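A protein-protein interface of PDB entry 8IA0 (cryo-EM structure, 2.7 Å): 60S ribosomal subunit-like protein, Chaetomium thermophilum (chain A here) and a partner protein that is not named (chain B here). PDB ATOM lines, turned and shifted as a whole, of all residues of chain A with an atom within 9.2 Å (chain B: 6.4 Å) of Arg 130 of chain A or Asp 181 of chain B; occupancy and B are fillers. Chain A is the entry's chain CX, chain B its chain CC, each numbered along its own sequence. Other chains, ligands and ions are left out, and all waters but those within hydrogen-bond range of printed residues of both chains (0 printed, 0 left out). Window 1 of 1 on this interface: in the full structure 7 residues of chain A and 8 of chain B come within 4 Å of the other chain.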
ATOM      1  N   ASN A 102     -20.975  18.448  35.025  1.00  0.00           N
ATOM      2  CA  ASN A 102     -21.357  17.602  33.900  1.00  0.00           C
ATOM      3  C   ASN A 102     -20.948  18.219  32.569  1.00  0.00           C
ATOM      4  O   ASN A 102     -20.520  17.508  31.653  1.00  0.00           O
ATOM      5  CB  ASN A 102     -22.860  17.340  33.927  1.00  0.00           C
ATOM      6  CG  ASN A 102     -23.197  15.989  34.496  1.00  0.00           C
ATOM      7  OD1 ASN A 102     -22.644  14.971  34.088  1.00  0.00           O
ATOM      8  ND2 ASN A 102     -24.119  15.968  35.450  1.00  0.00           N
ATOM      9  N   THR A 103     -21.087  19.539  32.435  1.00  0.00           N
ATOM     10  CA  THR A 103     -20.709  20.198  31.190  1.00  0.00           C
ATOM     11  C   THR A 103     -19.216  20.061  30.929  1.00  0.00           C
ATOM     12  O   THR A 103     -18.797  19.735  29.812  1.00  0.00           O
ATOM     13  CB  THR A 103     -21.113  21.671  31.228  1.00  0.00           C
ATOM     14  OG1 THR A 103     -22.482  21.786  31.634  1.00  0.00           O
ATOM     15  CG2 THR A 103     -20.941  22.302  29.859  1.00  0.00           C
ATOM     16  N   ALA A 106     -18.372  16.397  29.963  1.00  0.00           N
ATOM     17  CA  ALA A 106     -18.752  15.975  28.618  1.00  0.00           C
ATOM     18  C   ALA A 106     -17.712  16.394  27.586  1.00  0.00           C
ATOM     19  O   ALA A 106     -17.392  15.626  26.673  1.00  0.00           O
ATOM     20  CB  ALA A 106     -20.124  16.541  28.259  1.00  0.00           C
ATOM     21  N   MET A 107     -17.182  17.613  27.708  1.00  0.00           N
ATOM     22  CA  MET A 107     -16.134  18.060  26.794  1.00  0.00           C
ATOM     23  C   MET A 107     -14.884  17.202  26.924  1.00  0.00           C
ATOM     24  O   MET A 107     -14.255  16.852  25.920  1.00  0.00           O
ATOM     25  CB  MET A 107     -15.792  19.525  27.057  1.00  0.00           C
ATOM     26  CG  MET A 107     -16.977  20.416  27.358  1.00  0.00           C
ATOM     27  SD  MET A 107     -17.351  21.528  25.997  1.00  0.00           S
ATOM     28  CE  MET A 107     -16.411  22.965  26.505  1.00  0.00           C
ATOM     29  N   ARG A 122     -21.304  10.411  16.129  1.00  0.00           N
ATOM     30  CA  ARG A 122     -20.702  11.729  16.293  1.00  0.00           C
ATOM     31  C   ARG A 122     -21.744  12.761  16.699  1.00  0.00           C
ATOM     32  O   ARG A 122     -21.478  13.625  17.542  1.00  0.00           O
ATOM     33  CB  ARG A 122     -20.004  12.155  15.003  1.00  0.00           C
ATOM     34  CG  ARG A 122     -18.511  11.894  14.994  1.00  0.00           C
ATOM     35  CD  ARG A 122     -17.822  12.664  13.878  1.00  0.00           C
ATOM     36  NE  ARG A 122     -18.534  12.553  12.611  1.00  0.00           N
ATOM     37  CZ  ARG A 122     -18.084  11.889  11.557  1.00  0.00           C
ATOM     38  NH1 ARG A 122     -16.921  11.259  11.581  1.00  0.00           N
ATOM     39  NH2 ARG A 122     -18.819  11.855  10.449  1.00  0.00           N
ATOM     40  N   ALA A 123     -22.936  12.690  16.104  1.00  0.00           N
ATOM     41  CA  ALA A 123     -23.995  13.633  16.445  1.00  0.00           C
ATOM     42  C   ALA A 123     -24.425  13.483  17.897  1.00  0.00           C
ATOM     43  O   ALA A 123     -24.647  14.482  18.592  1.00  0.00           O
ATOM     44  CB  ALA A 123     -25.187  13.441  15.511  1.00  0.00           C
ATOM     45  N   ARG A 124     -24.554  12.243  18.373  1.00  0.00           N
ATOM     46  CA  ARG A 124     -25.010  12.019  19.741  1.00  0.00           C
ATOM     47  C   ARG A 124     -24.010  12.560  20.754  1.00  0.00           C
ATOM     48  O   ARG A 124     -24.404  13.107  21.790  1.00  0.00           O
ATOM     49  CB  ARG A 124     -25.261  10.530  19.970  1.00  0.00           C
ATOM     50  CG  ARG A 124     -26.398   9.970  19.141  1.00  0.00           C
ATOM     51  CD  ARG A 124     -27.743  10.374  19.705  1.00  0.00           C
ATOM     52  NE  ARG A 124     -28.781  10.364  18.682  1.00  0.00           N
ATOM     53  CZ  ARG A 124     -29.585   9.338  18.443  1.00  0.00           C
ATOM     54  NH1 ARG A 124     -29.499   8.215  19.137  1.00  0.00           N
ATOM     55  NH2 ARG A 124     -30.500   9.442  17.483  1.00  0.00           N
ATOM     56  N   GLN A 125     -22.715  12.410  20.475  1.00  0.00           N
ATOM     57  CA  GLN A 125     -21.695  12.937  21.375  1.00  0.00           C
ATOM     58  C   GLN A 125     -21.778  14.457  21.464  1.00  0.00           C
ATOM     59  O   GLN A 125     -21.639  15.035  22.548  1.00  0.00           O
ATOM     60  CB  GLN A 125     -20.312  12.489  20.904  1.00  0.00           C
ATOM     61  CG  GLN A 125     -19.159  13.262  21.502  1.00  0.00           C
ATOM     62  CD  GLN A 125     -17.849  12.976  20.800  1.00  0.00           C
ATOM     63  OE1 GLN A 125     -17.111  13.892  20.439  1.00  0.00           O
ATOM     64  NE2 GLN A 125     -17.554  11.699  20.600  1.00  0.00           N
ATOM     65  N   LEU A 126     -22.000  15.121  20.330  1.00  0.00           N
ATOM     66  CA  LEU A 126     -22.191  16.568  20.350  1.00  0.00           C
ATOM     67  C   LEU A 126     -23.491  16.942  21.051  1.00  0.00           C
ATOM     68  O   LEU A 126     -23.559  17.959  21.750  1.00  0.00           O
ATOM     69  CB  LEU A 126     -22.183  17.123  18.926  1.00  0.00           C
ATOM     70  CG  LEU A 126     -20.859  17.123  18.163  1.00  0.00           C
ATOM     71  CD1 LEU A 126     -21.120  17.209  16.671  1.00  0.00           C
ATOM     72  CD2 LEU A 126     -19.981  18.271  18.619  1.00  0.00           C
ATOM     73  N   GLU A 127     -24.536  16.132  20.868  1.00  0.00           N
ATOM     74  CA  GLU A 127     -25.846  16.473  21.410  1.00  0.00           C
ATOM     75  C   GLU A 127     -25.865  16.393  22.932  1.00  0.00           C
ATOM     76  O   GLU A 127     -26.528  17.201  23.589  1.00  0.00           O
ATOM     77  CB  GLU A 127     -26.911  15.558  20.810  1.00  0.00           C
ATOM     78  CG  GLU A 127     -28.335  15.949  21.156  1.00  0.00           C
ATOM     79  CD  GLU A 127     -29.315  15.605  20.054  1.00  0.00           C
ATOM     80  OE1 GLU A 127     -28.922  15.667  18.870  1.00  0.00           O
ATOM     81  OE2 GLU A 127     -30.477  15.272  20.370  1.00  0.00           O
ATOM     82  N   GLU A 128     -25.149  15.427  23.510  1.00  0.00           N
ATOM     83  CA  GLU A 128     -25.145  15.303  24.964  1.00  0.00           C
ATOM     84  C   GLU A 128     -24.418  16.467  25.623  1.00  0.00           C
ATOM     85  O   GLU A 128     -24.725  16.818  26.767  1.00  0.00           O
ATOM     86  CB  GLU A 128     -24.526  13.969  25.383  1.00  0.00           C
ATOM     87  CG  GLU A 128     -23.035  13.848  25.127  1.00  0.00           C
ATOM     88  CD  GLU A 128     -22.505  12.461  25.431  1.00  0.00           C
ATOM     89  OE1 GLU A 128     -23.309  11.588  25.818  1.00  0.00           O
ATOM     90  OE2 GLU A 128     -21.284  12.244  25.282  1.00  0.00           O
ATOM     91  N   ILE A 129     -23.456  17.072  24.926  1.00  0.00           N
ATOM     92  CA  ILE A 129     -22.842  18.297  25.425  1.00  0.00           C
ATOM     93  C   ILE A 129     -23.837  19.447  25.369  1.00  0.00           C
ATOM     94  O   ILE A 129     -23.876  20.300  26.264  1.00  0.00           O
ATOM     95  CB  ILE A 129     -21.562  18.616  24.634  1.00  0.00           C
ATOM     96  CG1 ILE A 129     -20.615  17.416  24.648  1.00  0.00           C
ATOM     97  CG2 ILE A 129     -20.871  19.833  25.214  1.00  0.00           C
ATOM     98  CD1 ILE A 129     -19.253  17.709  24.076  1.00  0.00           C
ATOM     99  N   ARG A 130     -24.657  19.490  24.315  1.00  0.00           N
ATOM    100  CA  ARG A 130     -25.658  20.545  24.193  1.00  0.00           C
ATOM    101  C   ARG A 130     -26.691  20.461  25.309  1.00  0.00           C
ATOM    102  O   ARG A 130     -27.078  21.483  25.883  1.00  0.00           O
ATOM    103  CB  ARG A 130     -26.340  20.462  22.830  1.00  0.00           C
ATOM    104  CG  ARG A 130     -25.461  20.861  21.663  1.00  0.00           C
ATOM    105  CD  ARG A 130     -26.223  20.752  20.358  1.00  0.00           C
ATOM    106  NE  ARG A 130     -25.337  20.543  19.221  1.00  0.00           N
ATOM    107  CZ  ARG A 130     -25.642  19.806  18.163  1.00  0.00           C
ATOM    108  NH1 ARG A 130     -26.810  19.192  18.062  1.00  0.00           N
ATOM    109  NH2 ARG A 130     -24.757  19.683  17.181  1.00  0.00           N
ATOM    110  N   GLU A 131     -27.152  19.251  25.625  1.00  0.00           N
ATOM    111  CA  GLU A 131     -28.123  19.092  26.701  1.00  0.00           C
ATOM    112  C   GLU A 131     -27.495  19.386  28.057  1.00  0.00           C
ATOM    113  O   GLU A 131     -28.166  19.896  28.961  1.00  0.00           O
ATOM    114  CB  GLU A 131     -28.712  17.683  26.675  1.00  0.00           C
ATOM    115  CG  GLU A 131     -29.533  17.378  25.435  1.00  0.00           C
ATOM    116  CD  GLU A 131     -30.812  18.190  25.367  1.00  0.00           C
ATOM    117  OE1 GLU A 131     -31.384  18.491  26.435  1.00  0.00           O
ATOM    118  OE2 GLU A 131     -31.245  18.527  24.245  1.00  0.00           O
ATOM    119  N   ALA A 132     -26.211  19.065  28.219  1.00  0.00           N
ATOM    120  CA  ALA A 132     -25.512  19.419  29.448  1.00  0.00           C
ATOM    121  C   ALA A 132     -25.418  20.929  29.607  1.00  0.00           C
ATOM    122  O   ALA A 132     -25.590  21.457  30.712  1.00  0.00           O
ATOM    123  CB  ALA A 132     -24.121  18.788  29.463  1.00  0.00           C
ATOM    124  N   ARG A 133     -25.139  21.642  28.515  1.00  0.00           N
ATOM    125  CA  ARG A 133     -25.099  23.099  28.575  1.00  0.00           C
ATOM    126  C   ARG A 133     -26.472  23.674  28.887  1.00  0.00           C
ATOM    127  O   ARG A 133     -26.594  24.621  29.673  1.00  0.00           O
ATOM    128  CB  ARG A 133     -24.579  23.669  27.258  1.00  0.00           C
ATOM    129  CG  ARG A 133     -23.085  23.569  27.066  1.00  0.00           C
ATOM    130  CD  ARG A 133     -22.643  24.507  25.965  1.00  0.00           C
ATOM    131  NE  ARG A 133     -21.358  24.126  25.396  1.00  0.00           N
ATOM    132  CZ  ARG A 133     -20.187  24.588  25.807  1.00  0.00           C
ATOM    133  NH1 ARG A 133     -20.096  25.443  26.811  1.00  0.00           N
ATOM    134  NH2 ARG A 133     -19.080  24.183  25.194  1.00  0.00           N
ATOM    135  N   ARG A 134     -27.518  23.120  28.270  1.00  0.00           N
ATOM    136  CA  ARG A 134     -28.865  23.636  28.483  1.00  0.00           C
ATOM    137  C   ARG A 134     -29.303  23.461  29.930  1.00  0.00           C
ATOM    138  O   ARG A 134     -29.914  24.363  30.516  1.00  0.00           O
ATOM    139  CB  ARG A 134     -29.843  22.941  27.538  1.00  0.00           C
ATOM    140  CG  ARG A 134     -31.064  23.771  27.190  1.00  0.00           C
ATOM    141  CD  ARG A 134     -32.145  22.926  26.520  1.00  0.00           C
ATOM    142  NE  ARG A 134     -32.428  21.659  27.193  1.00  0.00           N
ATOM    143  CZ  ARG A 134     -32.726  21.512  28.479  1.00  0.00           C
ATOM    144  NH1 ARG A 134     -32.879  22.552  29.282  1.00  0.00           N
ATOM    145  NH2 ARG A 134     -32.901  20.288  28.966  1.00  0.00           N
ATOM    146  N   ILE A 135     -29.007  22.305  30.523  1.00  0.00           N
ATOM    147  CA  ILE A 135     -29.376  22.066  31.915  1.00  0.00           C
ATOM    148  C   ILE A 135     -28.623  23.018  32.836  1.00  0.00           C
ATOM    149  O   ILE A 135     -29.195  23.566  33.785  1.00  0.00           O
ATOM    150  CB  ILE A 135     -29.123  20.594  32.285  1.00  0.00           C
ATOM    151  CG1 ILE A 135     -30.143  19.691  31.594  1.00  0.00           C
ATOM    152  CG2 ILE A 135     -29.190  20.400  33.789  1.00  0.00           C
ATOM    153  CD1 ILE A 135     -29.748  18.234  31.568  1.00  0.00           C
ATOM    154  N   GLU A 136     -27.331  23.228  32.573  1.00  0.00           N
ATOM    155  CA  GLU A 136     -26.550  24.152  33.389  1.00  0.00           C
ATOM    156  C   GLU A 136     -27.085  25.573  33.281  1.00  0.00           C
ATOM    157  O   GLU A 136     -27.188  26.283  34.288  1.00  0.00           O
ATOM    158  CB  GLU A 136     -25.081  24.104  32.974  1.00  0.00           C
ATOM    159  CG  GLU A 136     -24.188  25.011  33.794  1.00  0.00           C
ATOM    160  CD  GLU A 136     -22.762  25.035  33.289  1.00  0.00           C
ATOM    161  OE1 GLU A 136     -22.486  24.388  32.258  1.00  0.00           O
ATOM    162  OE2 GLU A 136     -21.915  25.701  33.922  1.00  0.00           O
ATOM    163  N   ALA A 137     -27.424  26.010  32.066  1.00  0.00           N
ATOM    164  CA  ALA A 137     -27.975  27.348  31.893  1.00  0.00           C
ATOM    165  C   ALA A 137     -29.326  27.479  32.581  1.00  0.00           C
ATOM    166  O   ALA A 137     -29.626  28.514  33.188  1.00  0.00           O
ATOM    167  CB  ALA A 137     -28.093  27.678  30.405  1.00  0.00           C
ATOM    168  N   GLU A 138     -30.160  26.442  32.491  1.00  0.00           N
ATOM    169  CA  GLU A 138     -31.440  26.455  33.188  1.00  0.00           C
ATOM    170  C   GLU A 138     -31.246  26.492  34.697  1.00  0.00           C
ATOM    171  O   GLU A 138     -31.955  27.217  35.405  1.00  0.00           O
ATOM    172  CB  GLU A 138     -32.268  25.237  32.784  1.00  0.00           C
ATOM    173  CG  GLU A 138     -33.657  25.199  33.393  1.00  0.00           C
ATOM    174  CD  GLU A 138     -34.503  24.069  32.842  1.00  0.00           C
ATOM    175  OE1 GLU A 138     -33.997  23.307  31.991  1.00  0.00           O
ATOM    176  OE2 GLU A 138     -35.674  23.943  33.257  1.00  0.00           O
ATOM    177  N   LEU B 177     -19.361  26.848  10.449  1.00  0.00           N
ATOM    178  CA  LEU B 177     -20.329  26.396  11.435  1.00  0.00           C
ATOM    179  C   LEU B 177     -19.737  25.402  12.424  1.00  0.00           C
ATOM    180  O   LEU B 177     -20.490  24.774  13.174  1.00  0.00           O
ATOM    181  CB  LEU B 177     -21.541  25.775  10.739  1.00  0.00           C
ATOM    182  CG  LEU B 177     -22.534  26.755  10.116  1.00  0.00           C
ATOM    183  CD1 LEU B 177     -23.685  26.009   9.465  1.00  0.00           C
ATOM    184  CD2 LEU B 177     -23.048  27.725  11.161  1.00  0.00           C
ATOM    185  N   SER B 178     -18.412  25.228  12.425  1.00  0.00           N
ATOM    186  CA  SER B 178     -17.776  24.407  13.449  1.00  0.00           C
ATOM    187  C   SER B 178     -17.953  25.017  14.832  1.00  0.00           C
ATOM    188  O   SER B 178     -18.137  24.288  15.810  1.00  0.00           O
ATOM    189  CB  SER B 178     -16.294  24.218  13.132  1.00  0.00           C
ATOM    190  OG  SER B 178     -16.108  23.861  11.773  1.00  0.00           O
ATOM    191  N   PHE B 179     -17.884  26.340  14.937  1.00  0.00           N
ATOM    192  CA  PHE B 179     -18.390  27.001  16.123  1.00  0.00           C
ATOM    193  C   PHE B 179     -19.890  26.752  16.229  1.00  0.00           C
ATOM    194  O   PHE B 179     -20.579  26.541  15.227  1.00  0.00           O
ATOM    195  CB  PHE B 179     -18.102  28.502  16.077  1.00  0.00           C
ATOM    196  CG  PHE B 179     -16.742  28.848  15.541  1.00  0.00           C
ATOM    197  CD1 PHE B 179     -15.649  28.915  16.384  1.00  0.00           C
ATOM    198  CD2 PHE B 179     -16.558  29.115  14.197  1.00  0.00           C
ATOM    199  CE1 PHE B 179     -14.398  29.234  15.898  1.00  0.00           C
ATOM    200  CE2 PHE B 179     -15.308  29.435  13.706  1.00  0.00           C
ATOM    201  CZ  PHE B 179     -14.229  29.494  14.558  1.00  0.00           C
ATOM    202  N   TYR B 180     -20.391  26.762  17.463  1.00  0.00           N
ATOM    203  CA  TYR B 180     -21.755  26.397  17.840  1.00  0.00           C
ATOM    204  C   TYR B 180     -22.003  24.897  17.762  1.00  0.00           C
ATOM    205  O   TYR B 180     -23.144  24.467  17.958  1.00  0.00           O
ATOM    206  CB  TYR B 180     -22.833  27.095  16.996  1.00  0.00           C
ATOM    207  CG  TYR B 180     -22.743  28.602  16.935  1.00  0.00           C
ATOM    208  CD1 TYR B 180     -23.391  29.391  17.869  1.00  0.00           C
ATOM    209  CD2 TYR B 180     -22.038  29.234  15.924  1.00  0.00           C
ATOM    210  CE1 TYR B 180     -23.324  30.764  17.810  1.00  0.00           C
ATOM    211  CE2 TYR B 180     -21.965  30.606  15.859  1.00  0.00           C
ATOM    212  CZ  TYR B 180     -22.611  31.366  16.802  1.00  0.00           C
ATOM    213  OH  TYR B 180     -22.541  32.735  16.742  1.00  0.00           O
ATOM    214  N   ASP B 181     -20.982  24.086  17.478  1.00  0.00           N
ATOM    215  CA  ASP B 181     -21.190  22.646  17.365  1.00  0.00           C
ATOM    216  C   ASP B 181     -21.651  22.045  18.687  1.00  0.00           C
ATOM    217  O   ASP B 181     -22.549  21.196  18.710  1.00  0.00           O
ATOM    218  CB  ASP B 181     -19.909  21.963  16.890  1.00  0.00           C
ATOM    219  CG  ASP B 181     -20.142  21.047  15.708  1.00  0.00           C
ATOM    220  OD1 ASP B 181     -21.293  20.968  15.232  1.00  0.00           O
ATOM    221  OD2 ASP B 181     -19.172  20.405  15.253  1.00  0.00           O
ATOM    222  N   SER B 182     -21.050  22.473  19.796  1.00  0.00           N
ATOM    223  CA  SER B 182     -21.403  21.985  21.122  1.00  0.00           C
ATOM    224  C   SER B 182     -22.290  22.961  21.882  1.00  0.00           C
ATOM    225  O   SER B 182     -22.182  23.071  23.107  1.00  0.00           O
ATOM    226  CB  SER B 182     -20.138  21.685  21.924  1.00  0.00           C
ATOM    227  OG  SER B 182     -19.239  22.776  21.875  1.00  0.00           O
ATOM    228  N   TYR B 183     -23.170  23.670  21.185  1.00  0.00           N
ATOM    229  CA  TYR B 183     -23.989  24.686  21.821  1.00  0.00           C
ATOM    230  C   TYR B 183     -25.458  24.455  21.511  1.00  0.00           C
ATOM    231  O   TYR B 183     -25.804  24.016  20.410  1.00  0.00           O
ATOM    232  CB  TYR B 183     -23.579  26.091  21.357  1.00  0.00           C
ATOM    233  CG  TYR B 183     -22.283  26.573  21.964  1.00  0.00           C
ATOM    234  CD1 TYR B 183     -21.066  26.271  21.376  1.00  0.00           C
ATOM    235  CD2 TYR B 183     -22.278  27.328  23.125  1.00  0.00           C
ATOM    236  CE1 TYR B 183     -19.883  26.705  21.926  1.00  0.00           C
ATOM    237  CE2 TYR B 183     -21.096  27.768  23.682  1.00  0.00           C
ATOM    238  CZ  TYR B 183     -19.903  27.455  23.078  1.00  0.00           C
ATOM    239  OH  TYR B 183     -18.720  27.888  23.627  1.00  0.00           O
ATOM    240  N   PRO B 184     -26.345  24.738  22.468  1.00  0.00           N
ATOM    241  CA  PRO B 184     -27.783  24.567  22.209  1.00  0.00           C
ATOM    242  C   PRO B 184     -28.325  25.519  21.162  1.00  0.00           C
ATOM    243  O   PRO B 184     -29.395  25.252  20.603  1.00  0.00           O
ATOM    244  CB  PRO B 184     -28.427  24.828  23.579  1.00  0.00           C
ATOM    245  CG  PRO B 184     -27.298  24.875  24.562  1.00  0.00           C
ATOM    246  CD  PRO B 184     -26.089  25.290  23.805  1.00  0.00           C
ATOM    247  N   HIS B 185     -27.631  26.616  20.882  1.00  0.00           N
ATOM    248  CA  HIS B 185     -28.091  27.636  19.955  1.00  0.00           C
ATOM    249  C   HIS B 185     -27.197  27.676  18.724  1.00  0.00           C
ATOM    250  O   HIS B 185     -26.070  27.175  18.726  1.00  0.00           O
ATOM    251  CB  HIS B 185     -28.112  29.011  20.627  1.00  0.00           C
ATOM    252  CG  HIS B 185     -26.754  29.542  20.954  1.00  0.00           C
ATOM    253  ND1 HIS B 185     -26.202  30.625  20.306  1.00  0.00           N
ATOM    254  CD2 HIS B 185     -25.833  29.138  21.859  1.00  0.00           C
ATOM    255  CE1 HIS B 185     -25.001  30.866  20.798  1.00  0.00           C
ATOM    256  NE2 HIS B 185     -24.752  29.977  21.741  1.00  0.00           N
ATOM    257  N   ARG B 197     -31.467  25.702  18.157  1.00  0.00           N
ATOM    258  CA  ARG B 197     -31.591  24.593  17.228  1.00  0.00           C
ATOM    259  C   ARG B 197     -33.008  24.027  17.289  1.00  0.00           C
ATOM    260  O   ARG B 197     -33.565  23.862  18.378  1.00  0.00           O
ATOM    261  CB  ARG B 197     -30.573  23.504  17.556  1.00  0.00           C
ATOM    262  CG  ARG B 197     -29.143  24.001  17.614  1.00  0.00           C
ATOM    263  CD  ARG B 197     -28.164  22.921  17.205  1.00  0.00           C
ATOM    264  NE  ARG B 197     -26.789  23.399  17.219  1.00  0.00           N
ATOM    265  CZ  ARG B 197     -25.848  22.984  16.382  1.00  0.00           C
ATOM    266  NH1 ARG B 197     -26.102  22.083  15.450  1.00  0.00           N
ATOM    267  NH2 ARG B 197     -24.623  23.488  16.484  1.00  0.00           N
ATOM    268  N   THR B 200     -34.042  17.440  16.938  1.00  0.00           N
ATOM    269  CA  THR B 200     -33.159  16.381  16.474  1.00  0.00           C
ATOM    270  C   THR B 200     -33.987  15.308  15.781  1.00  0.00           C
ATOM    271  O   THR B 200     -34.935  14.776  16.367  1.00  0.00           O
ATOM    272  CB  THR B 200     -32.370  15.769  17.633  1.00  0.00           C
ATOM    273  OG1 THR B 200     -31.575  16.783  18.259  1.00  0.00           O
ATOM    274  CG2 THR B 200     -31.464  14.655  17.129  1.00  0.00           C
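The guanidinium group (NE) of Arg 197 of chain B is in hydrogen-bond range of the backbone carbonyl oxygen (O) of Tyr 183 of chain B (3.4 Å).
The backbone NH (N) of Arg 197 of chain B sits at hydrogen-bond distance from the backbone carbonyl oxygen (O) of Pro 184 of chain B, 3.2 Å away.
The side-chain sulfur (SD) of Met 107 of chain A sits close to the guanidinium group (NH2) of Arg 133 of chain A, 3.3 Å away.
Asn 102 of chain A touches none of the printed residues of chain B.
Printed residues of chain B within 4 Å of Leu 126 of chain A: Asp 181.
Glu 128 of chain A touches none of the printed residues of chain B.
Of chain B, only Asp 181, Ser 182, Tyr 183, Pro 184 and Arg 197 come within 4 Å of Arg 130 of chain A.
Printed residues of chain B within 4 Å of Arg 133 of chain A: Ser 182 and Tyr 183.
Asp 181 of chain B touches just these residues of chain A: Leu 126 (3.9 Å) and Arg 130 (2.9 Å).
Ser 182 of chain B touches just these residues of chain A: Ile 129, Arg 130 and Arg 133.
Of the printed residues of chain A, Tyr 183 of chain B touches Arg 130 and Arg 133.
Of the printed residues of chain A, Arg 197 of chain B touches Arg 130 (3.3 Å).
Printed residues of chain A within 4 Å of Thr 200 of chain B: Glu 127.
The nearest printed residue of chain B that does not touch Leu 126 of chain A is Ser 182 of chain B (4.5 Å).
NE of Arg 130 of chain A is in hydrogen-bond range of O of Asp 181 of chain B (2.9 Å).
The backbone carbonyl oxygen of Ser 182 of chain B sits at hydrogen-bond distance from the guanidinium group of Arg 133 of chain A (2.7 Å).
The guanidinium group (NH2) of Arg 130 of chain A lies close to the guanidinium group (NH1) of Arg 197 of chain B (3.3 Å).
The side-chain carboxylate of Glu 127 of chain A lies within hydrogen-bond range of the side-chain hydroxyl of Thr 200 of chain B (2.8 Å).
Leu 126 of chain A touches Asp 181 of chain B (CD2 to O, 3.9 Å).
Ser 182 of chain B touches Ile 129 of chain A.
Ser 182 of chain B touches Arg 130 of chain A (C to CG, 3.8 Å).
Arg 130 of chain A touches Tyr 183 of chain B.
O of Arg 130 of chain A touches CG of Pro 184 of chain B (3.6 Å).
CZ of Arg 133 of chain A touches CE2 of Tyr 183 of chain B (3.9 Å).
Of the 21 printed residues of chain A, 5 touch a printed residue of chain B.
Hydrophobic or aromatic side chains of chain A within 4 Å of the printed part of chain B: Leu 126 and Ile 129.
Of the 11 printed residues of chain B, 6 touch a printed residue of chain A.
Among the printed residues, 10 pairs touch across the chains.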
